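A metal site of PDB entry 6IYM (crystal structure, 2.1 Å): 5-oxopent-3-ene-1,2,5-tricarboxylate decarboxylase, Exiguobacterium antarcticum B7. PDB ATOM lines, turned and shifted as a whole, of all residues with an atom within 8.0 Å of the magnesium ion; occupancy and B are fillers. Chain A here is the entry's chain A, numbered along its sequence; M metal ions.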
ATOM      1  N   CYS A  74     -16.545 -16.552  23.792  1.00  0.00           N
ATOM      2  CA  CYS A  74     -17.196 -17.536  24.686  1.00  0.00           C
ATOM      3  C   CYS A  74     -16.666 -17.432  26.118  1.00  0.00           C
ATOM      4  O   CYS A  74     -15.442 -17.389  26.320  1.00  0.00           O
ATOM      5  CB  CYS A  74     -16.956 -18.958  24.185  1.00  0.00           C
ATOM      6  SG  CYS A  74     -17.709 -19.285  22.571  1.00  0.00           S
ATOM      7  N   VAL A  75     -17.588 -17.445  27.080  1.00  0.00           N
ATOM      8  CA  VAL A  75     -17.307 -17.450  28.536  1.00  0.00           C
ATOM      9  C   VAL A  75     -17.192 -18.904  28.976  1.00  0.00           C
ATOM     10  O   VAL A  75     -17.950 -19.737  28.462  1.00  0.00           O
ATOM     11  CB  VAL A  75     -18.393 -16.677  29.309  1.00  0.00           C
ATOM     12  CG1 VAL A  75     -18.142 -16.727  30.813  1.00  0.00           C
ATOM     13  CG2 VAL A  75     -18.443 -15.234  28.819  1.00  0.00           C
ATOM     14  N   GLY A  76     -16.278 -19.199  29.917  1.00  0.00           N
ATOM     15  CA  GLY A  76     -16.143 -20.540  30.517  1.00  0.00           C
ATOM     16  C   GLY A  76     -17.247 -20.794  31.546  1.00  0.00           C
ATOM     17  O   GLY A  76     -18.343 -20.237  31.402  1.00  0.00           O
ATOM     18  N   LYS A  77     -16.991 -21.577  32.589  1.00  0.00           N
ATOM     19  CA  LYS A  77     -17.966 -21.852  33.682  1.00  0.00           C
ATOM     20  C   LYS A  77     -18.568 -20.516  34.162  1.00  0.00           C
ATOM     21  O   LYS A  77     -17.820 -19.679  34.704  1.00  0.00           O
ATOM     22  CB  LYS A  77     -17.269 -22.568  34.844  1.00  0.00           C
ATOM     23  CG  LYS A  77     -17.195 -24.078  34.716  1.00  0.00           C
ATOM     24  CD  LYS A  77     -16.812 -24.567  33.329  1.00  0.00           C
ATOM     25  CE  LYS A  77     -17.069 -26.047  33.144  1.00  0.00           C
ATOM     26  NZ  LYS A  77     -16.799 -26.461  31.751  1.00  0.00           N
ATOM     27  N   ASN A  78     -19.877 -20.334  33.987  1.00  0.00           N
ATOM     28  CA  ASN A  78     -20.580 -19.088  34.342  1.00  0.00           C
ATOM     29  C   ASN A  78     -21.898 -19.367  35.047  1.00  0.00           C
ATOM     30  O   ASN A  78     -22.678 -18.426  35.173  1.00  0.00           O
ATOM     31  CB  ASN A  78     -20.805 -18.208  33.130  1.00  0.00           C
ATOM     32  CG  ASN A  78     -21.038 -16.768  33.533  1.00  0.00           C
ATOM     33  OD1 ASN A  78     -20.459 -16.302  34.518  1.00  0.00           O
ATOM     34  ND2 ASN A  78     -21.905 -16.075  32.803  1.00  0.00           N
ATOM     35  N   PHE A  97     -12.625 -17.642  25.540  1.00  0.00           N
ATOM     36  CA  PHE A  97     -12.045 -18.340  24.355  1.00  0.00           C
ATOM     37  C   PHE A  97     -12.974 -18.097  23.165  1.00  0.00           C
ATOM     38  O   PHE A  97     -14.056 -17.463  23.344  1.00  0.00           O
ATOM     39  CB  PHE A  97     -11.849 -19.831  24.651  1.00  0.00           C
ATOM     40  CG  PHE A  97     -13.075 -20.456  25.242  1.00  0.00           C
ATOM     41  CD1 PHE A  97     -13.279 -20.453  26.610  1.00  0.00           C
ATOM     42  CD2 PHE A  97     -14.052 -20.989  24.414  1.00  0.00           C
ATOM     43  CE1 PHE A  97     -14.431 -21.003  27.150  1.00  0.00           C
ATOM     44  CE2 PHE A  97     -15.201 -21.533  24.961  1.00  0.00           C
ATOM     45  CZ  PHE A  97     -15.389 -21.546  26.320  1.00  0.00           C
ATOM     46  N   LYS A  99     -14.696 -19.383  19.072  1.00  0.00           N
ATOM     47  CA  LYS A  99     -15.100 -20.394  18.073  1.00  0.00           C
ATOM     48  C   LYS A  99     -14.966 -19.770  16.689  1.00  0.00           C
ATOM     49  O   LYS A  99     -15.541 -18.704  16.504  1.00  0.00           O
ATOM     50  CB  LYS A  99     -16.552 -20.813  18.304  1.00  0.00           C
ATOM     51  CG  LYS A  99     -16.781 -21.616  19.574  1.00  0.00           C
ATOM     52  CD  LYS A  99     -18.230 -21.738  19.898  1.00  0.00           C
ATOM     53  CE  LYS A  99     -18.886 -22.917  19.212  1.00  0.00           C
ATOM     54  NZ  LYS A  99     -18.433 -24.206  19.812  1.00  0.00           N
ATOM     55  N   TYR A 123     -22.749 -31.063  24.121  1.00  0.00           N
ATOM     56  CA  TYR A 123     -23.598 -29.873  23.915  1.00  0.00           C
ATOM     57  C   TYR A 123     -23.322 -28.842  25.025  1.00  0.00           C
ATOM     58  O   TYR A 123     -22.840 -29.172  26.140  1.00  0.00           O
ATOM     59  CB  TYR A 123     -25.088 -30.260  23.897  1.00  0.00           C
ATOM     60  CG  TYR A 123     -25.499 -31.057  25.113  1.00  0.00           C
ATOM     61  CD1 TYR A 123     -25.914 -30.447  26.275  1.00  0.00           C
ATOM     62  CD2 TYR A 123     -25.364 -32.430  25.134  1.00  0.00           C
ATOM     63  CE1 TYR A 123     -26.243 -31.180  27.404  1.00  0.00           C
ATOM     64  CE2 TYR A 123     -25.680 -33.193  26.253  1.00  0.00           C
ATOM     65  CZ  TYR A 123     -26.108 -32.557  27.401  1.00  0.00           C
ATOM     66  OH  TYR A 123     -26.377 -33.298  28.522  1.00  0.00           O
ATOM     67  N   GLU A 124     -23.674 -27.583  24.749  1.00  0.00           N
ATOM     68  CA  GLU A 124     -23.761 -26.491  25.767  1.00  0.00           C
ATOM     69  C   GLU A 124     -24.739 -25.455  25.242  1.00  0.00           C
ATOM     70  O   GLU A 124     -24.405 -24.758  24.272  1.00  0.00           O
ATOM     71  CB  GLU A 124     -22.411 -25.809  26.013  1.00  0.00           C
ATOM     72  CG  GLU A 124     -21.368 -26.654  26.711  1.00  0.00           C
ATOM     73  CD  GLU A 124     -20.111 -25.926  27.206  1.00  0.00           C
ATOM     74  OE1 GLU A 124     -19.284 -26.590  27.826  1.00  0.00           O
ATOM     75  OE2 GLU A 124     -19.943 -24.709  26.923  1.00  0.00           O
ATOM     76  N   GLY A 125     -25.915 -25.361  25.851  1.00  0.00           N
ATOM     77  CA  GLY A 125     -26.938 -24.366  25.472  1.00  0.00           C
ATOM     78  C   GLY A 125     -26.627 -23.045  26.089  1.00  0.00           C
ATOM     79  O   GLY A 125     -26.240 -23.040  27.287  1.00  0.00           O
ATOM     80  N   GLU A 126     -26.706 -21.946  25.339  1.00  0.00           N
ATOM     81  CA  GLU A 126     -26.157 -20.629  25.822  1.00  0.00           C
ATOM     82  C   GLU A 126     -26.940 -19.426  25.281  1.00  0.00           C
ATOM     83  O   GLU A 126     -27.377 -19.433  24.094  1.00  0.00           O
ATOM     84  CB  GLU A 126     -24.682 -20.521  25.456  1.00  0.00           C
ATOM     85  CG  GLU A 126     -23.796 -21.607  26.036  1.00  0.00           C
ATOM     86  CD  GLU A 126     -22.288 -21.330  26.102  1.00  0.00           C
ATOM     87  OE1 GLU A 126     -21.871 -20.143  25.913  1.00  0.00           O
ATOM     88  OE2 GLU A 126     -21.516 -22.287  26.434  1.00  0.00           O
ATOM     89  N   ILE A 153     -26.777 -19.744  21.154  1.00  0.00           N
ATOM     90  CA  ILE A 153     -25.600 -20.490  20.667  1.00  0.00           C
ATOM     91  C   ILE A 153     -25.624 -21.858  21.335  1.00  0.00           C
ATOM     92  O   ILE A 153     -25.880 -21.911  22.528  1.00  0.00           O
ATOM     93  CB  ILE A 153     -24.309 -19.702  21.008  1.00  0.00           C
ATOM     94  CG1 ILE A 153     -24.196 -18.464  20.130  1.00  0.00           C
ATOM     95  CG2 ILE A 153     -23.077 -20.585  20.895  1.00  0.00           C
ATOM     96  CD1 ILE A 153     -23.757 -18.776  18.755  1.00  0.00           C
ATOM     97  N   ASN A 154     -25.365 -22.915  20.559  1.00  0.00           N
ATOM     98  CA  ASN A 154     -24.977 -24.242  21.085  1.00  0.00           C
ATOM     99  C   ASN A 154     -23.462 -24.334  20.933  1.00  0.00           C
ATOM    100  O   ASN A 154     -22.981 -24.485  19.765  1.00  0.00           O
ATOM    101  CB  ASN A 154     -25.736 -25.376  20.399  1.00  0.00           C
ATOM    102  CG  ASN A 154     -25.590 -26.712  21.110  1.00  0.00           C
ATOM    103  OD1 ASN A 154     -24.718 -26.888  21.966  1.00  0.00           O
ATOM    104  ND2 ASN A 154     -26.358 -27.682  20.665  1.00  0.00           N
ATOM    105  N   ASP A 155     -22.743 -24.224  22.044  1.00  0.00           N
ATOM    106  CA  ASP A 155     -21.257 -24.264  22.082  1.00  0.00           C
ATOM    107  C   ASP A 155     -20.886 -25.741  22.019  1.00  0.00           C
ATOM    108  O   ASP A 155     -20.464 -26.295  23.037  1.00  0.00           O
ATOM    109  CB  ASP A 155     -20.707 -23.515  23.306  1.00  0.00           C
ATOM    110  CG  ASP A 155     -19.194 -23.599  23.540  1.00  0.00           C
ATOM    111  OD1 ASP A 155     -18.465 -24.048  22.645  1.00  0.00           O
ATOM    112  OD2 ASP A 155     -18.742 -23.226  24.668  1.00  0.00           O
ATOM    113  N   VAL A 156     -21.081 -26.368  20.871  1.00  0.00           N
ATOM    114  CA  VAL A 156     -20.755 -27.807  20.679  1.00  0.00           C
ATOM    115  C   VAL A 156     -19.243 -27.962  20.899  1.00  0.00           C
ATOM    116  O   VAL A 156     -18.482 -27.076  20.459  1.00  0.00           O
ATOM    117  CB  VAL A 156     -21.202 -28.350  19.303  1.00  0.00           C
ATOM    118  CG1 VAL A 156     -20.763 -29.791  19.099  1.00  0.00           C
ATOM    119  CG2 VAL A 156     -22.688 -28.212  19.070  1.00  0.00           C
ATOM    120  N   THR A 157     -18.817 -29.021  21.591  1.00  0.00           N
ATOM    121  CA  THR A 157     -17.461 -29.195  22.140  1.00  0.00           C
ATOM    122  C   THR A 157     -17.018 -30.665  22.037  1.00  0.00           C
ATOM    123  O   THR A 157     -17.808 -31.562  22.379  1.00  0.00           O
ATOM    124  CB  THR A 157     -17.429 -28.782  23.621  1.00  0.00           C
ATOM    125  OG1 THR A 157     -17.891 -27.446  23.821  1.00  0.00           O
ATOM    126  CG2 THR A 157     -16.041 -28.932  24.217  1.00  0.00           C
ATOM    127  N   ARG A 159     -14.769 -32.824  24.011  1.00  0.00           N
ATOM    128  CA  ARG A 159     -14.150 -32.810  25.362  1.00  0.00           C
ATOM    129  C   ARG A 159     -12.716 -33.388  25.325  1.00  0.00           C
ATOM    130  O   ARG A 159     -11.882 -32.916  26.133  1.00  0.00           O
ATOM    131  CB  ARG A 159     -15.047 -33.580  26.341  1.00  0.00           C
ATOM    132  CG  ARG A 159     -16.451 -32.999  26.482  1.00  0.00           C
ATOM    133  CD  ARG A 159     -16.405 -31.615  27.094  1.00  0.00           C
ATOM    134  NE  ARG A 159     -17.738 -31.047  27.253  1.00  0.00           N
ATOM    135  CZ  ARG A 159     -17.992 -29.779  27.623  1.00  0.00           C
ATOM    136  NH1 ARG A 159     -16.995 -28.940  27.860  1.00  0.00           N
ATOM    137  NH2 ARG A 159     -19.240 -29.363  27.738  1.00  0.00           N
ATOM    138  N   GLN A 162     -10.315 -30.774  23.701  1.00  0.00           N
ATOM    139  CA  GLN A 162     -10.102 -29.707  24.719  1.00  0.00           C
ATOM    140  C   GLN A 162      -8.818 -29.980  25.497  1.00  0.00           C
ATOM    141  O   GLN A 162      -8.056 -29.040  25.740  1.00  0.00           O
ATOM    142  CB  GLN A 162     -11.261 -29.616  25.711  1.00  0.00           C
ATOM    143  CG  GLN A 162     -12.272 -28.533  25.421  1.00  0.00           C
ATOM    144  CD  GLN A 162     -13.284 -28.461  26.547  1.00  0.00           C
ATOM    145  OE1 GLN A 162     -13.991 -29.423  26.845  1.00  0.00           O
ATOM    146  NE2 GLN A 162     -13.337 -27.329  27.223  1.00  0.00           N
ATOM    147  N   PHE A 168      -9.047 -24.262  24.427  1.00  0.00           N
ATOM    148  CA  PHE A 168     -10.365 -24.829  24.037  1.00  0.00           C
ATOM    149  C   PHE A 168     -10.645 -24.637  22.532  1.00  0.00           C
ATOM    150  O   PHE A 168     -11.476 -25.392  22.005  1.00  0.00           O
ATOM    151  CB  PHE A 168     -11.464 -24.251  24.939  1.00  0.00           C
ATOM    152  CG  PHE A 168     -11.342 -24.627  26.391  1.00  0.00           C
ATOM    153  CD1 PHE A 168     -10.518 -25.660  26.796  1.00  0.00           C
ATOM    154  CD2 PHE A 168     -12.091 -23.959  27.341  1.00  0.00           C
ATOM    155  CE1 PHE A 168     -10.407 -25.985  28.148  1.00  0.00           C
ATOM    156  CE2 PHE A 168     -11.997 -24.295  28.681  1.00  0.00           C
ATOM    157  CZ  PHE A 168     -11.151 -25.315  29.082  1.00  0.00           C
ATOM    158  N   LYS A 172     -13.615 -26.659  20.010  1.00  0.00           N
ATOM    159  CA  LYS A 172     -14.900 -25.902  19.936  1.00  0.00           C
ATOM    160  C   LYS A 172     -15.148 -25.380  18.511  1.00  0.00           C
ATOM    161  O   LYS A 172     -16.195 -24.758  18.308  1.00  0.00           O
ATOM    162  CB  LYS A 172     -14.910 -24.782  20.976  1.00  0.00           C
ATOM    163  CG  LYS A 172     -15.000 -25.324  22.398  1.00  0.00           C
ATOM    164  CD  LYS A 172     -15.120 -24.331  23.494  1.00  0.00           C
ATOM    165  CE  LYS A 172     -15.357 -24.993  24.847  1.00  0.00           C
ATOM    166  NZ  LYS A 172     -16.793 -25.114  25.204  1.00  0.00           N
ATOM    167  N   ALA A 238     -21.082 -15.565  23.712  1.00  0.00           N
ATOM    168  CA  ALA A 238     -21.752 -16.737  24.302  1.00  0.00           C
ATOM    169  C   ALA A 238     -21.509 -16.708  25.817  1.00  0.00           C
ATOM    170  O   ALA A 238     -20.365 -16.740  26.195  1.00  0.00           O
ATOM    171  CB  ALA A 238     -21.245 -17.980  23.660  1.00  0.00           C
ATOM    172  N   THR A 239     -22.571 -16.639  26.647  1.00  0.00           N
ATOM    173  CA  THR A 239     -22.474 -16.199  28.063  1.00  0.00           C
ATOM    174  C   THR A 239     -22.385 -17.379  29.031  1.00  0.00           C
ATOM    175  O   THR A 239     -22.548 -17.132  30.246  1.00  0.00           O
ATOM    176  CB  THR A 239     -23.606 -15.237  28.445  1.00  0.00           C
ATOM    177  OG1 THR A 239     -24.847 -15.896  28.224  1.00  0.00           O
ATOM    178  CG2 THR A 239     -23.586 -13.962  27.622  1.00  0.00           C
ATOM    179  N   GLY A 240     -22.057 -18.568  28.526  1.00  0.00           N
ATOM    180  CA  GLY A 240     -21.874 -19.803  29.305  1.00  0.00           C
ATOM    181  C   GLY A 240     -23.147 -20.642  29.330  1.00  0.00           C
ATOM    182  O   GLY A 240     -24.165 -20.195  28.777  1.00  0.00           O
ATOM    183  N   THR A 241     -23.116 -21.781  29.998  1.00  0.00           N
ATOM    184  CA  THR A 241     -24.110 -22.857  29.914  1.00  0.00           C
ATOM    185  C   THR A 241     -24.526 -23.293  31.299  1.00  0.00           C
ATOM    186  O   THR A 241     -23.706 -23.331  32.208  1.00  0.00           O
ATOM    187  CB  THR A 241     -23.529 -23.991  29.075  1.00  0.00           C
ATOM    188  OG1 THR A 241     -24.670 -24.711  28.599  1.00  0.00           O
ATOM    189  CG2 THR A 241     -22.544 -24.870  29.825  1.00  0.00           C
ATOM    190  N   VAL A 245     -24.418 -30.663  31.246  1.00  0.00           N
ATOM    191  CA  VAL A 245     -23.498 -30.996  30.120  1.00  0.00           C
ATOM    192  C   VAL A 245     -23.200 -32.500  30.125  1.00  0.00           C
ATOM    193  O   VAL A 245     -23.033 -33.081  31.216  1.00  0.00           O
ATOM    194  CB  VAL A 245     -22.264 -30.075  30.278  1.00  0.00           C
ATOM    195  CG1 VAL A 245     -20.928 -30.767  30.133  1.00  0.00           C
ATOM    196  CG2 VAL A 245     -22.387 -28.862  29.382  1.00  0.00           C
HETATM  197 MG    MG M   1     -19.596 -22.775  26.519  1.00  0.00          MG
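The side-chain carboxylate (OE1) of Glu 126 is in hydrogen-bond range of the backbone NH (N) of Gly 240, at 3.1 Å. The backbone NH of Glu 126 is in hydrogen-bond range of the backbone carbonyl oxygen of Ile 153, 2.9 Å away. OE1 of Glu 124 is in salt-bridge range of NH2 of Arg 159 (2.8 Å). The backbone NH of Glu 124 sits at hydrogen-bond distance from the side-chain amide oxygen of Asn 154 (3.1 Å). The side-chain carboxylate (OD1) of Asp 155 is in salt-bridge range of the side-chain amino group (NZ) of Lys 99, 2.8 Å away. OG1 of Thr 157 lies within hydrogen-bond range of NZ of Lys 172. O of Lys 172 lies within hydrogen-bond range of NZ of Lys 99, at 2.8 Å. N of Val 75 sits at hydrogen-bond distance from O of Ala 238 (3.0 Å).
Val 75 touches the magnesium ion (O to MG, 3.96 Å). NZ of Lys 172 touches the magnesium ion (3.9 Å). Of the 25 residues printed, 5 come within 4 Å of the magnesium ion.
The magnesium ion is bound by the side-chain carboxylate (OE2) of Glu 126 (2.0 Å), the side-chain carboxylate (OE2) of Glu 124 (2.0 Å) and the side-chain carboxylate (OD2) of Asp 155 (2.1 Å).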
